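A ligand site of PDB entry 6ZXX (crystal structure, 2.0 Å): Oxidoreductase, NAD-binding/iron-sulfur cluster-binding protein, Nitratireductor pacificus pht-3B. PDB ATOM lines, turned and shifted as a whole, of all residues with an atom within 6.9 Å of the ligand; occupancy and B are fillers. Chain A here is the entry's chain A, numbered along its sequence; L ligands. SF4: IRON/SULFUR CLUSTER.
Ser 499 touches the ligand. Arg 500 touches the ligand. CG1 of Ile 501 touches S2 of the ligand, 3.7 Å away. CD1 of Leu 506 touches FE3 of the ligand (3.9 Å). Phe 538 touches the ligand (CD1 to S1, 3.7 Å). Pro 596 touches the ligand (CD to S4, 3.4 Å). Trp 597 touches the ligand (CD1 to S1, 3.6 Å). Hydrophobic or aromatic side chains that line the ligand: Ile 501, Leu 506, Phe 538, Pro 596 and Trp 597. Of the 26 residues printed, 11 come within 4 Å of the ligand. Along chain A the residues within 4 Å of the ligand span positions 499 to 597. The nearest printed residue that does not touch the ligand is Lys 544 (4.1 Å).
The side-chain sulfur (SG) of Cys 595 binds an iron atom (FE3) of the ligand (2.2 Å). SG of Cys 539 binds FE4 of the ligand. SG of Cys 542 binds FE2 of the ligand, 2.2 Å away. A sulfur (S4) of the ligand lies close to the backbone NH (N) of Cys 545 (3.6 Å). FE1 of the ligand is bound by SG of Cys 545 (2.2 Å).
The backbone NH (N) of Trp 597 lies close to the side-chain sulfur (SG) of Cys 595 (3.4 Å). O of Cys 539 sits at hydrogen-bond distance from NH2 of Arg 500 (2.7 Å). O of Cys 542 is in hydrogen-bond range of NE of Arg 500, 3.1 Å away. The backbone NH (N) of Lys 544 lies close to the side-chain sulfur (SG) of Cys 542 (3.7 Å). The side-chain hydroxyl of Ser 499 lies close to the backbone NH of Ile 501, at 3.3 Å.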
ATOM      1  N   VAL A 498     -18.448  -0.017 -13.940  1.00  0.00           N
ATOM      2  CA  VAL A 498     -17.512  -0.839 -14.668  1.00  0.00           C
ATOM      3  C   VAL A 498     -16.115  -0.690 -14.020  1.00  0.00           C
ATOM      4  O   VAL A 498     -15.657   0.416 -13.799  1.00  0.00           O
ATOM      5  CB  VAL A 498     -17.495  -0.440 -16.178  1.00  0.00           C
ATOM      6  CG1 VAL A 498     -16.208  -0.845 -16.895  1.00  0.00           C
ATOM      7  CG2 VAL A 498     -18.698  -1.030 -16.901  1.00  0.00           C
ATOM      8  N   SER A 499     -15.448  -1.825 -13.747  1.00  0.00           N
ATOM      9  CA  SER A 499     -14.101  -1.831 -13.199  1.00  0.00           C
ATOM     10  C   SER A 499     -13.131  -2.538 -14.128  1.00  0.00           C
ATOM     11  O   SER A 499     -13.553  -3.195 -15.092  1.00  0.00           O
ATOM     12  CB  SER A 499     -14.080  -2.574 -11.872  1.00  0.00           C
ATOM     13  OG  SER A 499     -14.270  -3.959 -12.057  1.00  0.00           O
ATOM     14  N   ARG A 500     -11.831  -2.454 -13.812  1.00  0.00           N
ATOM     15  CA  ARG A 500     -10.823  -3.141 -14.648  1.00  0.00           C
ATOM     16  C   ARG A 500     -10.947  -4.635 -14.582  1.00  0.00           C
ATOM     17  O   ARG A 500     -10.581  -5.345 -15.535  1.00  0.00           O
ATOM     18  CB  ARG A 500      -9.418  -2.739 -14.285  1.00  0.00           C
ATOM     19  CG  ARG A 500      -8.294  -3.427 -15.035  1.00  0.00           C
ATOM     20  CD  ARG A 500      -6.923  -2.892 -14.590  1.00  0.00           C
ATOM     21  NE  ARG A 500      -6.848  -1.456 -14.815  1.00  0.00           N
ATOM     22  CZ  ARG A 500      -6.657  -0.865 -16.006  1.00  0.00           C
ATOM     23  NH1 ARG A 500      -6.441  -1.566 -17.106  1.00  0.00           N
ATOM     24  NH2 ARG A 500      -6.611   0.458 -16.067  1.00  0.00           N
ATOM     25  N   ILE A 501     -11.495  -5.155 -13.490  1.00  0.00           N
ATOM     26  CA  ILE A 501     -11.583  -6.604 -13.347  1.00  0.00           C
ATOM     27  C   ILE A 501     -12.238  -7.203 -14.606  1.00  0.00           C
ATOM     28  O   ILE A 501     -11.820  -8.238 -15.103  1.00  0.00           O
ATOM     29  CB  ILE A 501     -12.328  -7.003 -12.047  1.00  0.00           C
ATOM     30  CG1 ILE A 501     -11.499  -6.514 -10.862  1.00  0.00           C
ATOM     31  CG2 ILE A 501     -12.501  -8.533 -11.981  1.00  0.00           C
ATOM     32  CD1 ILE A 501     -12.112  -6.745  -9.485  1.00  0.00           C
ATOM     33  N   GLY A 502     -13.312  -6.564 -15.066  1.00  0.00           N
ATOM     34  CA  GLY A 502     -13.866  -6.812 -16.369  1.00  0.00           C
ATOM     35  C   GLY A 502     -15.304  -7.271 -16.437  1.00  0.00           C
ATOM     36  O   GLY A 502     -16.172  -6.565 -16.978  1.00  0.00           O
ATOM     37  N   LEU A 506     -18.065  -2.818  -9.667  1.00  0.00           N
ATOM     38  CA  LEU A 506     -17.478  -2.519  -8.393  1.00  0.00           C
ATOM     39  C   LEU A 506     -18.373  -1.509  -7.675  1.00  0.00           C
ATOM     40  O   LEU A 506     -18.810  -0.501  -8.214  1.00  0.00           O
ATOM     41  CB  LEU A 506     -16.046  -2.011  -8.628  1.00  0.00           C
ATOM     42  CG  LEU A 506     -15.123  -1.769  -7.455  1.00  0.00           C
ATOM     43  CD1 LEU A 506     -13.692  -1.890  -7.908  1.00  0.00           C
ATOM     44  CD2 LEU A 506     -15.372  -0.436  -6.791  1.00  0.00           C
ATOM     45  N   PRO A 512     -15.564  -4.878  -5.188  1.00  0.00           N
ATOM     46  CA  PRO A 512     -16.009  -5.996  -6.103  1.00  0.00           C
ATOM     47  C   PRO A 512     -16.423  -7.281  -5.371  1.00  0.00           C
ATOM     48  O   PRO A 512     -16.700  -8.274  -6.031  1.00  0.00           O
ATOM     49  CB  PRO A 512     -14.765  -6.255  -6.940  1.00  0.00           C
ATOM     50  CG  PRO A 512     -13.643  -5.930  -6.020  1.00  0.00           C
ATOM     51  CD  PRO A 512     -14.098  -4.854  -5.060  1.00  0.00           C
ATOM     52  N   LEU A 535     -14.941   5.882 -10.388  1.00  0.00           N
ATOM     53  CA  LEU A 535     -14.176   4.641 -10.553  1.00  0.00           C
ATOM     54  C   LEU A 535     -13.383   4.602 -11.848  1.00  0.00           C
ATOM     55  O   LEU A 535     -12.305   4.033 -11.927  1.00  0.00           O
ATOM     56  CB  LEU A 535     -15.081   3.408 -10.485  1.00  0.00           C
ATOM     57  CG  LEU A 535     -14.249   2.140 -10.303  1.00  0.00           C
ATOM     58  CD1 LEU A 535     -13.501   2.099  -8.984  1.00  0.00           C
ATOM     59  CD2 LEU A 535     -15.165   0.946 -10.453  1.00  0.00           C
ATOM     60  N   PHE A 538     -10.211   6.233 -11.244  1.00  0.00           N
ATOM     61  CA  PHE A 538      -9.471   5.395 -10.299  1.00  0.00           C
ATOM     62  C   PHE A 538      -8.848   4.159 -10.971  1.00  0.00           C
ATOM     63  O   PHE A 538      -7.622   3.956 -10.880  1.00  0.00           O
ATOM     64  CB  PHE A 538     -10.385   4.946  -9.164  1.00  0.00           C
ATOM     65  CG  PHE A 538      -9.637   4.464  -7.970  1.00  0.00           C
ATOM     66  CD1 PHE A 538      -8.997   3.195  -7.972  1.00  0.00           C
ATOM     67  CD2 PHE A 538      -9.540   5.260  -6.830  1.00  0.00           C
ATOM     68  CE1 PHE A 538      -8.290   2.771  -6.834  1.00  0.00           C
ATOM     69  CE2 PHE A 538      -8.839   4.820  -5.703  1.00  0.00           C
ATOM     70  CZ  PHE A 538      -8.202   3.597  -5.713  1.00  0.00           C
ATOM     71  N   CYS A 539      -9.645   3.349 -11.647  1.00  0.00           N
ATOM     72  CA  CYS A 539      -9.122   2.156 -12.346  1.00  0.00           C
ATOM     73  C   CYS A 539      -8.115   2.509 -13.433  1.00  0.00           C
ATOM     74  O   CYS A 539      -7.232   1.711 -13.719  1.00  0.00           O
ATOM     75  CB  CYS A 539     -10.235   1.272 -12.932  1.00  0.00           C
ATOM     76  SG  CYS A 539     -11.151   0.251 -11.731  1.00  0.00           S
ATOM     77  N   ASN A 540      -8.278   3.656 -14.074  1.00  0.00           N
ATOM     78  CA  ASN A 540      -7.307   4.118 -15.081  1.00  0.00           C
ATOM     79  C   ASN A 540      -5.909   4.258 -14.542  1.00  0.00           C
ATOM     80  O   ASN A 540      -4.952   4.044 -15.289  1.00  0.00           O
ATOM     81  CB  ASN A 540      -7.752   5.406 -15.795  1.00  0.00           C
ATOM     82  CG  ASN A 540      -8.826   5.118 -16.890  1.00  0.00           C
ATOM     83  OD1 ASN A 540      -8.822   4.066 -17.585  1.00  0.00           O
ATOM     84  ND2 ASN A 540      -9.770   6.049 -17.040  1.00  0.00           N
ATOM     85  N   GLN A 541      -5.777   4.523 -13.237  1.00  0.00           N
ATOM     86  CA  GLN A 541      -4.434   4.603 -12.662  1.00  0.00           C
ATOM     87  C   GLN A 541      -4.101   3.504 -11.682  1.00  0.00           C
ATOM     88  O   GLN A 541      -3.141   3.598 -10.930  1.00  0.00           O
ATOM     89  CB  GLN A 541      -4.181   5.985 -12.056  1.00  0.00           C
ATOM     90  CG  GLN A 541      -5.346   6.614 -11.365  1.00  0.00           C
ATOM     91  CD  GLN A 541      -5.141   8.076 -11.064  1.00  0.00           C
ATOM     92  OE1 GLN A 541      -4.001   8.573 -10.892  1.00  0.00           O
ATOM     93  NE2 GLN A 541      -6.240   8.776 -10.907  1.00  0.00           N
ATOM     94  N   CYS A 542      -4.852   2.428 -11.702  1.00  0.00           N
ATOM     95  CA  CYS A 542      -4.574   1.263 -10.850  1.00  0.00           C
ATOM     96  C   CYS A 542      -4.443   0.034 -11.765  1.00  0.00           C
ATOM     97  O   CYS A 542      -5.019   0.010 -12.839  1.00  0.00           O
ATOM     98  CB  CYS A 542      -5.720   1.075  -9.865  1.00  0.00           C
ATOM     99  SG  CYS A 542      -5.570  -0.244  -8.647  1.00  0.00           S
ATOM    100  N   ARG A 543      -3.637  -0.947 -11.366  1.00  0.00           N
ATOM    101  CA  ARG A 543      -3.474  -2.233 -12.084  1.00  0.00           C
ATOM    102  C   ARG A 543      -3.391  -3.419 -11.132  1.00  0.00           C
ATOM    103  O   ARG A 543      -2.958  -4.493 -11.516  1.00  0.00           O
ATOM    104  CB  ARG A 543      -2.171  -2.213 -12.887  1.00  0.00           C
ATOM    105  CG  ARG A 543      -2.030  -1.072 -13.869  1.00  0.00           C
ATOM    106  CD  ARG A 543      -2.987  -1.262 -15.028  1.00  0.00           C
ATOM    107  NE  ARG A 543      -2.815  -0.290 -16.111  1.00  0.00           N
ATOM    108  CZ  ARG A 543      -3.200   0.994 -16.057  1.00  0.00           C
ATOM    109  NH1 ARG A 543      -3.730   1.526 -14.966  1.00  0.00           N
ATOM    110  NH2 ARG A 543      -3.011   1.764 -17.106  1.00  0.00           N
ATOM    111  N   LYS A 544      -3.827  -3.259  -9.887  1.00  0.00           N
ATOM    112  CA  LYS A 544      -3.484  -4.229  -8.875  1.00  0.00           C
ATOM    113  C   LYS A 544      -4.064  -5.589  -9.151  1.00  0.00           C
ATOM    114  O   LYS A 544      -3.383  -6.616  -9.044  1.00  0.00           O
ATOM    115  CB  LYS A 544      -3.886  -3.720  -7.486  1.00  0.00           C
ATOM    116  CG  LYS A 544      -3.453  -4.616  -6.356  1.00  0.00           C
ATOM    117  CD  LYS A 544      -3.367  -3.892  -5.032  1.00  0.00           C
ATOM    118  CE  LYS A 544      -2.929  -4.869  -3.952  1.00  0.00           C
ATOM    119  NZ  LYS A 544      -2.652  -4.084  -2.710  1.00  0.00           N
ATOM    120  N   CYS A 545      -5.345  -5.595  -9.509  1.00  0.00           N
ATOM    121  CA  CYS A 545      -6.069  -6.835  -9.859  1.00  0.00           C
ATOM    122  C   CYS A 545      -5.423  -7.551 -11.035  1.00  0.00           C
ATOM    123  O   CYS A 545      -5.172  -8.751 -10.999  1.00  0.00           O
ATOM    124  CB  CYS A 545      -7.538  -6.526 -10.147  1.00  0.00           C
ATOM    125  SG  CYS A 545      -7.814  -5.334 -11.483  1.00  0.00           S
ATOM    126  N   ALA A 546      -5.117  -6.756 -12.051  1.00  0.00           N
ATOM    127  CA  ALA A 546      -4.394  -7.242 -13.257  1.00  0.00           C
ATOM    128  C   ALA A 546      -3.053  -7.927 -12.929  1.00  0.00           C
ATOM    129  O   ALA A 546      -2.719  -9.007 -13.484  1.00  0.00           O
ATOM    130  CB  ALA A 546      -4.146  -6.079 -14.215  1.00  0.00           C
ATOM    131  N   ILE A 554      -6.680 -10.346 -16.711  1.00  0.00           N
ATOM    132  CA  ILE A 554      -7.230  -9.033 -16.551  1.00  0.00           C
ATOM    133  C   ILE A 554      -6.376  -8.088 -17.418  1.00  0.00           C
ATOM    134  O   ILE A 554      -5.150  -8.135 -17.411  1.00  0.00           O
ATOM    135  CB  ILE A 554      -7.326  -8.622 -15.075  1.00  0.00           C
ATOM    136  CG1 ILE A 554      -8.320  -9.486 -14.352  1.00  0.00           C
ATOM    137  CG2 ILE A 554      -7.781  -7.160 -14.931  1.00  0.00           C
ATOM    138  CD1 ILE A 554      -8.473  -9.207 -12.863  1.00  0.00           C
ATOM    139  N   TRP A 568     -13.678  -2.888 -19.778  1.00  0.00           N
ATOM    140  CA  TRP A 568     -12.343  -3.494 -19.738  1.00  0.00           C
ATOM    141  C   TRP A 568     -12.539  -4.968 -19.958  1.00  0.00           C
ATOM    142  O   TRP A 568     -13.069  -5.650 -19.107  1.00  0.00           O
ATOM    143  CB  TRP A 568     -11.659  -3.284 -18.410  1.00  0.00           C
ATOM    144  CG  TRP A 568     -10.899  -2.016 -18.287  1.00  0.00           C
ATOM    145  CD1 TRP A 568      -9.689  -1.712 -18.870  1.00  0.00           C
ATOM    146  CD2 TRP A 568     -11.263  -0.866 -17.518  1.00  0.00           C
ATOM    147  NE1 TRP A 568      -9.292  -0.452 -18.498  1.00  0.00           N
ATOM    148  CE2 TRP A 568     -10.244   0.088 -17.666  1.00  0.00           C
ATOM    149  CE3 TRP A 568     -12.351  -0.556 -16.700  1.00  0.00           C
ATOM    150  CZ2 TRP A 568     -10.286   1.320 -17.019  1.00  0.00           C
ATOM    151  CZ3 TRP A 568     -12.387   0.680 -16.060  1.00  0.00           C
ATOM    152  CH2 TRP A 568     -11.353   1.595 -16.216  1.00  0.00           C
ATOM    153  N   CYS A 591      -8.981 -11.646  -7.639  1.00  0.00           N
ATOM    154  CA  CYS A 591      -9.082 -10.281  -8.167  1.00  0.00           C
ATOM    155  C   CYS A 591      -9.941  -9.398  -7.282  1.00  0.00           C
ATOM    156  O   CYS A 591      -9.627  -8.198  -7.083  1.00  0.00           O
ATOM    157  CB  CYS A 591      -9.613 -10.297  -9.580  1.00  0.00           C
ATOM    158  SG  CYS A 591     -11.077 -11.338  -9.849  1.00  0.00           S
ATOM    159  N   MET A 594      -7.788  -8.583  -4.070  1.00  0.00           N
ATOM    160  CA  MET A 594      -6.592  -7.711  -4.194  1.00  0.00           C
ATOM    161  C   MET A 594      -6.907  -6.237  -4.491  1.00  0.00           C
ATOM    162  O   MET A 594      -6.058  -5.346  -4.394  1.00  0.00           O
ATOM    163  CB  MET A 594      -5.641  -8.270  -5.238  1.00  0.00           C
ATOM    164  CG  MET A 594      -5.151  -9.673  -4.909  1.00  0.00           C
ATOM    165  SD  MET A 594      -4.453  -9.886  -3.256  1.00  0.00           S
ATOM    166  CE  MET A 594      -2.919  -8.965  -3.411  1.00  0.00           C
ATOM    167  N   CYS A 595      -8.177  -5.968  -4.770  1.00  0.00           N
ATOM    168  CA  CYS A 595      -8.625  -4.623  -5.110  1.00  0.00           C
ATOM    169  C   CYS A 595      -8.588  -3.715  -3.919  1.00  0.00           C
ATOM    170  O   CYS A 595      -9.026  -4.097  -2.837  1.00  0.00           O
ATOM    171  CB  CYS A 595     -10.065  -4.689  -5.642  1.00  0.00           C
ATOM    172  SG  CYS A 595     -10.743  -3.107  -6.118  1.00  0.00           S
ATOM    173  N   PRO A 596      -8.113  -2.471  -4.129  1.00  0.00           N
ATOM    174  CA  PRO A 596      -8.063  -1.528  -3.005  1.00  0.00           C
ATOM    175  C   PRO A 596      -9.418  -1.246  -2.387  1.00  0.00           C
ATOM    176  O   PRO A 596      -9.495  -0.986  -1.200  1.00  0.00           O
ATOM    177  CB  PRO A 596      -7.430  -0.275  -3.643  1.00  0.00           C
ATOM    178  CG  PRO A 596      -6.518  -0.837  -4.718  1.00  0.00           C
ATOM    179  CD  PRO A 596      -7.313  -1.976  -5.287  1.00  0.00           C
ATOM    180  N   TRP A 597     -10.465  -1.327  -3.184  1.00  0.00           N
ATOM    181  CA  TRP A 597     -11.793  -1.047  -2.695  1.00  0.00           C
ATOM    182  C   TRP A 597     -12.335  -2.205  -1.847  1.00  0.00           C
ATOM    183  O   TRP A 597     -13.383  -2.076  -1.170  1.00  0.00           O
ATOM    184  CB  TRP A 597     -12.736  -0.802  -3.830  1.00  0.00           C
ATOM    185  CG  TRP A 597     -12.463   0.429  -4.614  1.00  0.00           C
ATOM    186  CD1 TRP A 597     -11.560   0.584  -5.649  1.00  0.00           C
ATOM    187  CD2 TRP A 597     -13.126   1.711  -4.447  1.00  0.00           C
ATOM    188  NE1 TRP A 597     -11.637   1.874  -6.142  1.00  0.00           N
ATOM    189  CE2 TRP A 597     -12.554   2.594  -5.409  1.00  0.00           C
ATOM    190  CE3 TRP A 597     -14.120   2.189  -3.583  1.00  0.00           C
ATOM    191  CZ2 TRP A 597     -12.983   3.927  -5.538  1.00  0.00           C
ATOM    192  CZ3 TRP A 597     -14.514   3.508  -3.693  1.00  0.00           C
ATOM    193  CH2 TRP A 597     -13.943   4.363  -4.670  1.00  0.00           C
ATOM    194  N   ASN A 598     -11.611  -3.316  -1.857  1.00  0.00           N
ATOM    195  CA  ASN A 598     -11.918  -4.407  -0.948  1.00  0.00           C
ATOM    196  C   ASN A 598     -11.278  -4.085   0.390  1.00  0.00           C
ATOM    197  O   ASN A 598     -10.084  -4.335   0.608  1.00  0.00           O
ATOM    198  CB  ASN A 598     -11.417  -5.748  -1.495  1.00  0.00           C
ATOM    199  CG  ASN A 598     -11.702  -6.877  -0.548  1.00  0.00           C
ATOM    200  OD1 ASN A 598     -12.794  -6.990  -0.064  1.00  0.00           O
ATOM    201  ND2 ASN A 598     -10.697  -7.670  -0.230  1.00  0.00           N
ATOM    202  N   ILE A 623      -3.872   4.419  -4.174  1.00  0.00           N
ATOM    203  CA  ILE A 623      -3.498   3.244  -4.947  1.00  0.00           C
ATOM    204  C   ILE A 623      -2.112   2.720  -4.560  1.00  0.00           C
ATOM    205  O   ILE A 623      -1.926   1.514  -4.348  1.00  0.00           O
ATOM    206  CB  ILE A 623      -3.518   3.557  -6.447  1.00  0.00           C
ATOM    207  CG1 ILE A 623      -4.953   3.801  -6.890  1.00  0.00           C
ATOM    208  CG2 ILE A 623      -2.901   2.433  -7.229  1.00  0.00           C
ATOM    209  CD1 ILE A 623      -5.063   4.457  -8.232  1.00  0.00           C
HETATM  210 FE1  SF4 L   1      -8.570  -3.476 -10.468  1.00  0.00          FE
HETATM  211 FE2  SF4 L   1      -7.498  -1.255  -9.100  1.00  0.00          FE
HETATM  212 FE3  SF4 L   1      -9.868  -2.584  -8.053  1.00  0.00          FE
HETATM  213 FE4  SF4 L   1      -9.905  -1.007 -10.416  1.00  0.00          FE
HETATM  214  S1  SF4 L   1      -9.395  -0.482  -8.376  1.00  0.00           S
HETATM  215  S2  SF4 L   1     -10.617  -3.010 -10.061  1.00  0.00           S
HETATM  216  S3  SF4 L   1      -8.003  -1.562 -11.136  1.00  0.00           S
HETATM  217  S4  SF4 L   1      -7.883  -3.263  -8.409  1.00  0.00           S
